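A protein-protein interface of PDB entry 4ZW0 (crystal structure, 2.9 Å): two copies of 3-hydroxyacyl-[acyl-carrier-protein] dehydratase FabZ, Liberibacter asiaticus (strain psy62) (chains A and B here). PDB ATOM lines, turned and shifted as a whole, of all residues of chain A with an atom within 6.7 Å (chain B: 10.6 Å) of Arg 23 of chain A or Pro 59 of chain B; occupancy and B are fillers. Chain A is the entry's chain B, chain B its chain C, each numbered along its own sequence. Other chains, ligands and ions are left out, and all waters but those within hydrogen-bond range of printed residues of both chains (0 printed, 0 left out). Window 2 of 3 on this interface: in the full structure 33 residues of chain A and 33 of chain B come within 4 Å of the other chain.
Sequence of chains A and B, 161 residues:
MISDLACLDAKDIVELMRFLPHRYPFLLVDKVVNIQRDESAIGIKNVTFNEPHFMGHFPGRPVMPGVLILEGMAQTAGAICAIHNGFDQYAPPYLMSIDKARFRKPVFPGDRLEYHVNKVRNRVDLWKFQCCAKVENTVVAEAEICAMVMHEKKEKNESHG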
ATOM      1  N   LEU A  16      17.927 -24.353 -28.411  1.00  0.00           N
ATOM      2  CA  LEU A  16      16.730 -23.502 -28.559  1.00  0.00           C
ATOM      3  C   LEU A  16      16.108 -23.087 -27.218  1.00  0.00           C
ATOM      4  O   LEU A  16      15.792 -21.887 -26.994  1.00  0.00           O
ATOM      5  CB  LEU A  16      15.688 -24.226 -29.420  1.00  0.00           C
ATOM      6  CG  LEU A  16      16.009 -24.196 -30.896  1.00  0.00           C
ATOM      7  CD1 LEU A  16      14.978 -24.976 -31.724  1.00  0.00           C
ATOM      8  CD2 LEU A  16      16.059 -22.723 -31.254  1.00  0.00           C
ATOM      9  N   MET A  17      15.957 -24.077 -26.329  1.00  0.00           N
ATOM     10  CA  MET A  17      15.328 -23.839 -25.040  1.00  0.00           C
ATOM     11  C   MET A  17      16.015 -22.732 -24.236  1.00  0.00           C
ATOM     12  O   MET A  17      15.390 -22.104 -23.362  1.00  0.00           O
ATOM     13  CB  MET A  17      15.214 -25.151 -24.267  1.00  0.00           C
ATOM     14  CG  MET A  17      13.915 -25.922 -24.582  1.00  0.00           C
ATOM     15  SD  MET A  17      13.941 -27.712 -24.218  1.00  0.00           S
ATOM     16  CE  MET A  17      13.266 -27.691 -22.540  1.00  0.00           C
ATOM     17  N   ARG A  18      17.285 -22.458 -24.573  1.00  0.00           N
ATOM     18  CA  ARG A  18      18.050 -21.371 -23.928  1.00  0.00           C
ATOM     19  C   ARG A  18      17.697 -19.992 -24.436  1.00  0.00           C
ATOM     20  O   ARG A  18      17.938 -18.999 -23.741  1.00  0.00           O
ATOM     21  CB  ARG A  18      19.557 -21.571 -24.056  1.00  0.00           C
ATOM     22  CG  ARG A  18      20.043 -22.865 -23.452  1.00  0.00           C
ATOM     23  CD  ARG A  18      21.533 -23.035 -23.607  1.00  0.00           C
ATOM     24  NE  ARG A  18      21.914 -24.442 -23.486  1.00  0.00           N
ATOM     25  CZ  ARG A  18      22.608 -25.126 -24.404  1.00  0.00           C
ATOM     26  NH1 ARG A  18      23.022 -24.524 -25.525  1.00  0.00           N
ATOM     27  NH2 ARG A  18      22.900 -26.418 -24.197  1.00  0.00           N
ATOM     28  N   PHE A  19      17.122 -19.927 -25.637  1.00  0.00           N
ATOM     29  CA  PHE A  19      16.802 -18.628 -26.238  1.00  0.00           C
ATOM     30  C   PHE A  19      15.328 -18.367 -26.305  1.00  0.00           C
ATOM     31  O   PHE A  19      14.889 -17.213 -26.335  1.00  0.00           O
ATOM     32  CB  PHE A  19      17.458 -18.482 -27.622  1.00  0.00           C
ATOM     33  CG  PHE A  19      18.911 -18.856 -27.614  1.00  0.00           C
ATOM     34  CD1 PHE A  19      19.872 -17.953 -27.147  1.00  0.00           C
ATOM     35  CD2 PHE A  19      19.316 -20.138 -27.994  1.00  0.00           C
ATOM     36  CE1 PHE A  19      21.212 -18.310 -27.100  1.00  0.00           C
ATOM     37  CE2 PHE A  19      20.674 -20.510 -27.948  1.00  0.00           C
ATOM     38  CZ  PHE A  19      21.619 -19.596 -27.501  1.00  0.00           C
ATOM     39  N   LEU A  20      14.569 -19.461 -26.335  1.00  0.00           N
ATOM     40  CA  LEU A  20      13.109 -19.398 -26.260  1.00  0.00           C
ATOM     41  C   LEU A  20      12.645 -19.792 -24.870  1.00  0.00           C
ATOM     42  O   LEU A  20      13.025 -20.860 -24.368  1.00  0.00           O
ATOM     43  CB  LEU A  20      12.497 -20.295 -27.325  1.00  0.00           C
ATOM     44  CG  LEU A  20      12.811 -19.763 -28.734  1.00  0.00           C
ATOM     45  CD1 LEU A  20      12.401 -20.703 -29.824  1.00  0.00           C
ATOM     46  CD2 LEU A  20      12.104 -18.430 -28.932  1.00  0.00           C
ATOM     47  N   PRO A  21      11.864 -18.898 -24.232  1.00  0.00           N
ATOM     48  CA  PRO A  21      11.145 -19.223 -22.987  1.00  0.00           C
ATOM     49  C   PRO A  21      10.010 -20.291 -23.146  1.00  0.00           C
ATOM     50  O   PRO A  21       9.781 -21.044 -22.196  1.00  0.00           O
ATOM     51  CB  PRO A  21      10.572 -17.859 -22.550  1.00  0.00           C
ATOM     52  CG  PRO A  21      10.495 -17.000 -23.799  1.00  0.00           C
ATOM     53  CD  PRO A  21      11.521 -17.555 -24.760  1.00  0.00           C
ATOM     54  N   HIS A  22       9.348 -20.316 -24.314  1.00  0.00           N
ATOM     55  CA  HIS A  22       8.327 -21.262 -24.716  1.00  0.00           C
ATOM     56  C   HIS A  22       8.600 -22.706 -24.326  1.00  0.00           C
ATOM     57  O   HIS A  22       9.671 -23.244 -24.611  1.00  0.00           O
ATOM     58  CB  HIS A  22       8.176 -21.240 -26.252  1.00  0.00           C
ATOM     59  CG  HIS A  22       7.827 -19.901 -26.824  1.00  0.00           C
ATOM     60  ND1 HIS A  22       8.760 -18.911 -27.025  1.00  0.00           N
ATOM     61  CD2 HIS A  22       6.645 -19.395 -27.253  1.00  0.00           C
ATOM     62  CE1 HIS A  22       8.173 -17.852 -27.551  1.00  0.00           C
ATOM     63  NE2 HIS A  22       6.889 -18.122 -27.709  1.00  0.00           N
ATOM     64  N   ARG A  23       7.606 -23.368 -23.736  1.00  0.00           N
ATOM     65  CA  ARG A  23       7.734 -24.800 -23.481  1.00  0.00           C
ATOM     66  C   ARG A  23       6.515 -25.506 -23.969  1.00  0.00           C
ATOM     67  O   ARG A  23       5.582 -24.866 -24.452  1.00  0.00           O
ATOM     68  CB  ARG A  23       7.892 -25.005 -21.998  1.00  0.00           C
ATOM     69  CG  ARG A  23       9.164 -24.407 -21.463  1.00  0.00           C
ATOM     70  CD  ARG A  23      10.351 -25.123 -22.133  1.00  0.00           C
ATOM     71  NE  ARG A  23      11.653 -24.719 -21.591  1.00  0.00           N
ATOM     72  CZ  ARG A  23      12.370 -23.684 -22.032  1.00  0.00           C
ATOM     73  NH1 ARG A  23      11.934 -22.941 -23.033  1.00  0.00           N
ATOM     74  NH2 ARG A  23      13.519 -23.395 -21.459  1.00  0.00           N
ATOM     75  N   TYR A  24       6.511 -26.820 -23.857  1.00  0.00           N
ATOM     76  CA  TYR A  24       5.298 -27.575 -24.152  1.00  0.00           C
ATOM     77  C   TYR A  24       4.047 -27.024 -23.416  1.00  0.00           C
ATOM     78  O   TYR A  24       4.112 -26.743 -22.238  1.00  0.00           O
ATOM     79  CB  TYR A  24       5.525 -29.033 -23.804  1.00  0.00           C
ATOM     80  CG  TYR A  24       4.356 -29.932 -24.068  1.00  0.00           C
ATOM     81  CD1 TYR A  24       4.182 -30.538 -25.317  1.00  0.00           C
ATOM     82  CD2 TYR A  24       3.409 -30.190 -23.071  1.00  0.00           C
ATOM     83  CE1 TYR A  24       3.078 -31.381 -25.571  1.00  0.00           C
ATOM     84  CE2 TYR A  24       2.302 -31.011 -23.312  1.00  0.00           C
ATOM     85  CZ  TYR A  24       2.150 -31.610 -24.559  1.00  0.00           C
ATOM     86  OH  TYR A  24       1.078 -32.428 -24.780  1.00  0.00           O
ATOM     87  N   PRO A  25       2.893 -26.890 -24.113  1.00  0.00           N
ATOM     88  CA  PRO A  25       2.616 -27.288 -25.516  1.00  0.00           C
ATOM     89  C   PRO A  25       2.742 -26.185 -26.578  1.00  0.00           C
ATOM     90  O   PRO A  25       1.971 -26.135 -27.522  1.00  0.00           O
ATOM     91  CB  PRO A  25       1.167 -27.706 -25.436  1.00  0.00           C
ATOM     92  CG  PRO A  25       0.586 -26.607 -24.508  1.00  0.00           C
ATOM     93  CD  PRO A  25       1.663 -26.412 -23.444  1.00  0.00           C
ATOM     94  N   PHE A  26       3.729 -25.312 -26.444  1.00  0.00           N
ATOM     95  CA  PHE A  26       3.737 -24.126 -27.280  1.00  0.00           C
ATOM     96  C   PHE A  26       5.120 -23.788 -27.786  1.00  0.00           C
ATOM     97  O   PHE A  26       5.403 -22.644 -28.168  1.00  0.00           O
ATOM     98  CB  PHE A  26       3.151 -22.945 -26.529  1.00  0.00           C
ATOM     99  CG  PHE A  26       2.189 -22.179 -27.339  1.00  0.00           C
ATOM    100  CD1 PHE A  26       0.868 -22.589 -27.422  1.00  0.00           C
ATOM    101  CD2 PHE A  26       2.609 -21.067 -28.070  1.00  0.00           C
ATOM    102  CE1 PHE A  26      -0.036 -21.874 -28.232  1.00  0.00           C
ATOM    103  CE2 PHE A  26       1.725 -20.358 -28.864  1.00  0.00           C
ATOM    104  CZ  PHE A  26       0.396 -20.757 -28.958  1.00  0.00           C
ATOM    105  N   LEU A  27       5.987 -24.797 -27.765  1.00  0.00           N
ATOM    106  CA  LEU A  27       7.276 -24.678 -28.394  1.00  0.00           C
ATOM    107  C   LEU A  27       7.133 -25.359 -29.732  1.00  0.00           C
ATOM    108  O   LEU A  27       7.097 -26.600 -29.830  1.00  0.00           O
ATOM    109  CB  LEU A  27       8.357 -25.321 -27.553  1.00  0.00           C
ATOM    110  CG  LEU A  27       9.774 -25.210 -28.112  1.00  0.00           C
ATOM    111  CD1 LEU A  27      10.064 -23.817 -28.666  1.00  0.00           C
ATOM    112  CD2 LEU A  27      10.710 -25.516 -26.988  1.00  0.00           C
ATOM    113  N   LEU A  28       7.049 -24.526 -30.765  1.00  0.00           N
ATOM    114  CA  LEU A  28       6.613 -24.972 -32.077  1.00  0.00           C
ATOM    115  C   LEU A  28       7.693 -24.993 -33.173  1.00  0.00           C
ATOM    116  O   LEU A  28       7.367 -24.991 -34.355  1.00  0.00           O
ATOM    117  CB  LEU A  28       5.370 -24.174 -32.499  1.00  0.00           C
ATOM    118  CG  LEU A  28       4.202 -24.351 -31.504  1.00  0.00           C
ATOM    119  CD1 LEU A  28       2.969 -23.601 -31.936  1.00  0.00           C
ATOM    120  CD2 LEU A  28       3.846 -25.795 -31.236  1.00  0.00           C
ATOM    121  N   GLN A  89      15.978 -16.530 -23.084  1.00  0.00           N
ATOM    122  CA  GLN A  89      14.755 -16.481 -22.272  1.00  0.00           C
ATOM    123  C   GLN A  89      15.028 -15.604 -21.012  1.00  0.00           C
ATOM    124  O   GLN A  89      16.087 -14.968 -20.921  1.00  0.00           O
ATOM    125  CB  GLN A  89      14.303 -17.902 -21.909  1.00  0.00           C
ATOM    126  CG  GLN A  89      15.445 -18.917 -21.744  1.00  0.00           C
ATOM    127  CD  GLN A  89      15.161 -19.921 -20.640  1.00  0.00           C
ATOM    128  OE1 GLN A  89      14.014 -20.072 -20.211  1.00  0.00           O
ATOM    129  NE2 GLN A  89      16.208 -20.597 -20.154  1.00  0.00           N
ATOM    130  N   PHE B  49      -6.017 -19.266 -15.877  1.00  0.00           N
ATOM    131  CA  PHE B  49      -4.748 -19.955 -15.792  1.00  0.00           C
ATOM    132  C   PHE B  49      -4.823 -21.445 -16.160  1.00  0.00           C
ATOM    133  O   PHE B  49      -3.883 -22.006 -16.756  1.00  0.00           O
ATOM    134  CB  PHE B  49      -4.169 -19.794 -14.377  1.00  0.00           C
ATOM    135  CG  PHE B  49      -2.853 -20.471 -14.203  1.00  0.00           C
ATOM    136  CD1 PHE B  49      -1.711 -19.966 -14.837  1.00  0.00           C
ATOM    137  CD2 PHE B  49      -2.745 -21.639 -13.445  1.00  0.00           C
ATOM    138  CE1 PHE B  49      -0.481 -20.609 -14.718  1.00  0.00           C
ATOM    139  CE2 PHE B  49      -1.492 -22.301 -13.321  1.00  0.00           C
ATOM    140  CZ  PHE B  49      -0.367 -21.778 -13.961  1.00  0.00           C
ATOM    141  N   GLU B  51      -5.645 -23.286 -18.439  1.00  0.00           N
ATOM    142  CA  GLU B  51      -5.653 -23.684 -19.852  1.00  0.00           C
ATOM    143  C   GLU B  51      -4.290 -24.276 -20.181  1.00  0.00           C
ATOM    144  O   GLU B  51      -3.276 -23.880 -19.599  1.00  0.00           O
ATOM    145  CB  GLU B  51      -5.985 -22.494 -20.757  1.00  0.00           C
ATOM    146  CG  GLU B  51      -7.315 -21.819 -20.468  1.00  0.00           C
ATOM    147  CD  GLU B  51      -7.620 -20.619 -21.410  1.00  0.00           C
ATOM    148  OE1 GLU B  51      -7.725 -20.806 -22.658  1.00  0.00           O
ATOM    149  OE2 GLU B  51      -7.771 -19.478 -20.885  1.00  0.00           O
ATOM    150  N   PRO B  52      -4.267 -25.258 -21.084  1.00  0.00           N
ATOM    151  CA  PRO B  52      -3.051 -26.033 -21.402  1.00  0.00           C
ATOM    152  C   PRO B  52      -1.880 -25.231 -21.996  1.00  0.00           C
ATOM    153  O   PRO B  52      -0.706 -25.508 -21.668  1.00  0.00           O
ATOM    154  CB  PRO B  52      -3.558 -27.107 -22.378  1.00  0.00           C
ATOM    155  CG  PRO B  52      -4.879 -26.587 -22.869  1.00  0.00           C
ATOM    156  CD  PRO B  52      -5.464 -25.816 -21.728  1.00  0.00           C
ATOM    157  N   HIS B  53      -2.193 -24.228 -22.813  1.00  0.00           N
ATOM    158  CA  HIS B  53      -1.139 -23.395 -23.394  1.00  0.00           C
ATOM    159  C   HIS B  53      -0.296 -22.650 -22.380  1.00  0.00           C
ATOM    160  O   HIS B  53       0.891 -22.417 -22.613  1.00  0.00           O
ATOM    161  CB  HIS B  53      -1.657 -22.435 -24.476  1.00  0.00           C
ATOM    162  CG  HIS B  53      -2.876 -21.680 -24.093  1.00  0.00           C
ATOM    163  ND1 HIS B  53      -2.821 -20.477 -23.428  1.00  0.00           N
ATOM    164  CD2 HIS B  53      -4.185 -21.942 -24.309  1.00  0.00           C
ATOM    165  CE1 HIS B  53      -4.047 -20.026 -23.246  1.00  0.00           C
ATOM    166  NE2 HIS B  53      -4.893 -20.900 -23.764  1.00  0.00           N
ATOM    167  N   PHE B  54      -0.892 -22.303 -21.249  1.00  0.00           N
ATOM    168  CA  PHE B  54      -0.194 -21.583 -20.189  1.00  0.00           C
ATOM    169  C   PHE B  54       0.912 -22.366 -19.540  1.00  0.00           C
ATOM    170  O   PHE B  54       1.772 -21.760 -18.876  1.00  0.00           O
ATOM    171  CB  PHE B  54      -1.194 -21.058 -19.159  1.00  0.00           C
ATOM    172  CG  PHE B  54      -1.936 -19.853 -19.648  1.00  0.00           C
ATOM    173  CD1 PHE B  54      -1.241 -18.840 -20.317  1.00  0.00           C
ATOM    174  CD2 PHE B  54      -3.325 -19.742 -19.510  1.00  0.00           C
ATOM    175  CE1 PHE B  54      -1.938 -17.716 -20.793  1.00  0.00           C
ATOM    176  CE2 PHE B  54      -4.004 -18.629 -19.982  1.00  0.00           C
ATOM    177  CZ  PHE B  54      -3.314 -17.618 -20.624  1.00  0.00           C
ATOM    178  N   MET B  55       0.901 -23.692 -19.722  1.00  0.00           N
ATOM    179  CA  MET B  55       2.036 -24.519 -19.280  1.00  0.00           C
ATOM    180  C   MET B  55       3.374 -24.071 -19.917  1.00  0.00           C
ATOM    181  O   MET B  55       4.441 -24.191 -19.313  1.00  0.00           O
ATOM    182  CB  MET B  55       1.800 -25.961 -19.682  1.00  0.00           C
ATOM    183  CG  MET B  55       1.273 -26.899 -18.634  1.00  0.00           C
ATOM    184  SD  MET B  55       1.342 -28.639 -19.229  1.00  0.00           S
ATOM    185  CE  MET B  55       0.126 -28.651 -20.612  1.00  0.00           C
ATOM    186  N   GLY B  56       3.312 -23.584 -21.156  1.00  0.00           N
ATOM    187  CA  GLY B  56       4.511 -23.284 -21.890  1.00  0.00           C
ATOM    188  C   GLY B  56       4.576 -21.876 -22.434  1.00  0.00           C
ATOM    189  O   GLY B  56       5.483 -21.565 -23.194  1.00  0.00           O
ATOM    190  N   HIS B  57       3.629 -21.023 -22.063  1.00  0.00           N
ATOM    191  CA  HIS B  57       3.585 -19.679 -22.620  1.00  0.00           C
ATOM    192  C   HIS B  57       3.077 -18.625 -21.618  1.00  0.00           C
ATOM    193  O   HIS B  57       1.998 -18.036 -21.799  1.00  0.00           O
ATOM    194  CB  HIS B  57       2.753 -19.674 -23.902  1.00  0.00           C
ATOM    195  CG  HIS B  57       2.886 -18.428 -24.732  1.00  0.00           C
ATOM    196  ND1 HIS B  57       2.324 -17.219 -24.371  1.00  0.00           N
ATOM    197  CD2 HIS B  57       3.485 -18.210 -25.932  1.00  0.00           C
ATOM    198  CE1 HIS B  57       2.583 -16.314 -25.298  1.00  0.00           C
ATOM    199  NE2 HIS B  57       3.289 -16.890 -26.256  1.00  0.00           N
ATOM    200  N   PHE B  58       3.874 -18.355 -20.589  1.00  0.00           N
ATOM    201  CA  PHE B  58       5.196 -18.918 -20.450  1.00  0.00           C
ATOM    202  C   PHE B  58       5.294 -19.454 -19.077  1.00  0.00           C
ATOM    203  O   PHE B  58       4.577 -19.007 -18.193  1.00  0.00           O
ATOM    204  CB  PHE B  58       6.239 -17.823 -20.585  1.00  0.00           C
ATOM    205  CG  PHE B  58       6.342 -17.296 -21.936  1.00  0.00           C
ATOM    206  CD1 PHE B  58       5.708 -16.115 -22.272  1.00  0.00           C
ATOM    207  CD2 PHE B  58       7.043 -18.018 -22.905  1.00  0.00           C
ATOM    208  CE1 PHE B  58       5.743 -15.650 -23.573  1.00  0.00           C
ATOM    209  CE2 PHE B  58       7.089 -17.573 -24.231  1.00  0.00           C
ATOM    210  CZ  PHE B  58       6.430 -16.375 -24.560  1.00  0.00           C
ATOM    211  N   PRO B  59       6.211 -20.399 -18.876  1.00  0.00           N
ATOM    212  CA  PRO B  59       6.386 -20.969 -17.527  1.00  0.00           C
ATOM    213  C   PRO B  59       6.700 -19.895 -16.467  1.00  0.00           C
ATOM    214  O   PRO B  59       7.674 -19.160 -16.590  1.00  0.00           O
ATOM    215  CB  PRO B  59       7.543 -21.962 -17.685  1.00  0.00           C
ATOM    216  CG  PRO B  59       7.888 -22.010 -19.163  1.00  0.00           C
ATOM    217  CD  PRO B  59       6.904 -21.153 -19.935  1.00  0.00           C
ATOM    218  N   GLY B  60       5.840 -19.799 -15.458  1.00  0.00           N
ATOM    219  CA  GLY B  60       5.946 -18.799 -14.421  1.00  0.00           C
ATOM    220  C   GLY B  60       5.491 -17.416 -14.836  1.00  0.00           C
ATOM    221  O   GLY B  60       5.501 -16.497 -14.023  1.00  0.00           O
ATOM    222  N   ARG B  61       5.103 -17.250 -16.096  1.00  0.00           N
ATOM    223  CA  ARG B  61       4.650 -15.962 -16.587  1.00  0.00           C
ATOM    224  C   ARG B  61       3.618 -16.213 -17.666  1.00  0.00           C
ATOM    225  O   ARG B  61       3.876 -16.034 -18.874  1.00  0.00           O
ATOM    226  CB  ARG B  61       5.848 -15.150 -17.122  1.00  0.00           C
ATOM    227  CG  ARG B  61       5.638 -13.639 -17.238  1.00  0.00           C
ATOM    228  CD  ARG B  61       6.893 -12.942 -17.819  1.00  0.00           C
ATOM    229  NE  ARG B  61       7.034 -13.087 -19.277  1.00  0.00           N
ATOM    230  CZ  ARG B  61       6.420 -12.307 -20.172  1.00  0.00           C
ATOM    231  NH1 ARG B  61       5.610 -11.332 -19.752  1.00  0.00           N
ATOM    232  NH2 ARG B  61       6.598 -12.495 -21.483  1.00  0.00           N
ATOM    233  N   PRO B  62       2.430 -16.644 -17.234  1.00  0.00           N
ATOM    234  CA  PRO B  62       1.319 -16.897 -18.165  1.00  0.00           C
ATOM    235  C   PRO B  62       0.871 -15.622 -18.891  1.00  0.00           C
ATOM    236  O   PRO B  62       0.359 -14.655 -18.289  1.00  0.00           O
ATOM    237  CB  PRO B  62       0.185 -17.365 -17.239  1.00  0.00           C
ATOM    238  CG  PRO B  62       0.535 -16.789 -15.846  1.00  0.00           C
ATOM    239  CD  PRO B  62       2.042 -16.783 -15.814  1.00  0.00           C
ATOM    240  N   VAL B  63       1.061 -15.607 -20.198  1.00  0.00           N
ATOM    241  CA  VAL B  63       0.439 -14.560 -21.004  1.00  0.00           C
ATOM    242  C   VAL B  63      -0.162 -15.153 -22.276  1.00  0.00           C
ATOM    243  O   VAL B  63       0.478 -15.977 -22.926  1.00  0.00           O
ATOM    244  CB  VAL B  63       1.449 -13.445 -21.323  1.00  0.00           C
ATOM    245  CG1 VAL B  63       2.715 -14.026 -21.975  1.00  0.00           C
ATOM    246  CG2 VAL B  63       0.781 -12.348 -22.176  1.00  0.00           C
ATOM    247  N   MET B  64      -1.391 -14.742 -22.596  1.00  0.00           N
ATOM    248  CA  MET B  64      -2.160 -15.269 -23.753  1.00  0.00           C
ATOM    249  C   MET B  64      -1.470 -15.007 -25.074  1.00  0.00           C
ATOM    250  O   MET B  64      -1.145 -13.840 -25.387  1.00  0.00           O
ATOM    251  CB  MET B  64      -3.520 -14.597 -23.825  1.00  0.00           C
ATOM    252  CG  MET B  64      -4.315 -14.960 -25.022  1.00  0.00           C
ATOM    253  SD  MET B  64      -5.538 -16.204 -24.596  1.00  0.00           S
ATOM    254  CE  MET B  64      -6.621 -16.093 -26.003  1.00  0.00           C
ATOM    255  N   PRO B  65      -1.226 -16.090 -25.842  1.00  0.00           N
ATOM    256  CA  PRO B  65      -0.530 -16.016 -27.133  1.00  0.00           C
ATOM    257  C   PRO B  65      -1.415 -15.275 -28.126  1.00  0.00           C
ATOM    258  O   PRO B  65      -2.584 -15.680 -28.277  1.00  0.00           O
ATOM    259  CB  PRO B  65      -0.395 -17.490 -27.550  1.00  0.00           C
ATOM    260  CG  PRO B  65      -0.497 -18.245 -26.289  1.00  0.00           C
ATOM    261  CD  PRO B  65      -1.503 -17.481 -25.455  1.00  0.00           C
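N of Arg 23 of chain A lies within hydrogen-bond range of O of Gly 56 of chain B. The backbone NH (N) of Gly 56 of chain B lies within hydrogen-bond range of the backbone carbonyl oxygen (O) of Tyr 24 of chain A.
ND1 of His 57 of chain B lies within hydrogen-bond range of O of Val 63 of chain B, at 2.7 Å. NH1 of Arg 23 of chain A is in hydrogen-bond range of O of Leu 20 of chain A. The guanidinium group (NH1) of Arg 23 of chain A sits at hydrogen-bond distance from the backbone carbonyl oxygen (O) of Pro 21 of chain A. The backbone carbonyl oxygen (O) of Met 17 of chain A sits at hydrogen-bond distance from the guanidinium group (NH2) of Arg 23 of chain A, 3.0 Å away. OE1 of Glu 51 of chain B sits at hydrogen-bond distance from NE2 of His 53 of chain B (3.0 Å).
Among the printed residues, pairs that only touch across the chains: Pro 21 of chain A with Phe 58 of chain B (3.5 Å), Pro 21 of chain A with Pro 59 of chain B (3.7 Å), His 22 of chain A with Gly 56 of chain B (3.2 Å), His 22 of chain A with His 57 of chain B (3.6 Å), His 22 of chain A with Phe 58 of chain B (3.5 Å), Arg 23 of chain A with Pro 59 of chain B (3.6 Å), Tyr 24 of chain A with Met 55 of chain B (3.5 Å), Pro 25 of chain A with Pro 52 of chain B (3.1 Å), Pro 25 of chain A with His 53 of chain B (3.8 Å), Pro 25 of chain A with Met 55 of chain B (3.8 Å), Pro 25 of chain A with Gly 56 of chain B (3.99 Å), Phe 26 of chain A with His 53 of chain B (3.9 Å), Phe 26 of chain A with His 57 of chain B (3.7 Å) and Phe 26 of chain A with Pro 65 of chain B (3.6 Å).
Arg 23 of chain A touches just these residues of chain B: Gly 56 and Pro 59. Of chain A, only Pro 21 (3.7 Å) and Arg 23 (3.6 Å) come within 4 Å of Pro 59 of chain B. No residue of chain B comes within 4 Å of Met 17 of chain A. Of chain B, only Phe 58 and Pro 59 come within 4 Å of Pro 21 of chain A. Leu 27 of chain A touches none of the printed residues of chain B. Printed residues of chain A within 4 Å of His 53 of chain B: Pro 25 (3.8 Å) and Phe 26 (3.9 Å). Of the printed residues of chain A, Gly 56 of chain B touches His 22 (3.2 Å), Arg 23 (2.8 Å), Tyr 24 (3.4 Å) and Pro 25 (3.99 Å). The nearest residue of chain B that does not touch Arg 23 of chain A is Met 55 of chain B (4.4 Å). The nearest printed residue of chain B that does not touch Tyr 24 of chain A is Pro 52 of chain B (5.0 Å).
Printed residues of chain B that touch a printed residue of chain A: Pro 52, His 53, Met 55, Gly 56, His 57, Phe 58, Pro 59 and Pro 65. Hydrophobic or aromatic side chains of chain B that line the printed part of chain A: His 53, Met 55, His 57, Phe 58, Pro 59 and Pro 65. Hydrophobic or aromatic side chains of chain A that line the printed part of chain B: Pro 21, His 22, Pro 25 and Phe 26. Among the printed residues, no Asp or Glu carboxylate lies within 4 Å of a Lys or Arg side-chain nitrogen of the other chain.
No position is printed for both chains. Of the 16 pairs that touch across the chains among the printed residues, none has its exchanged pair printed and touching as well.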
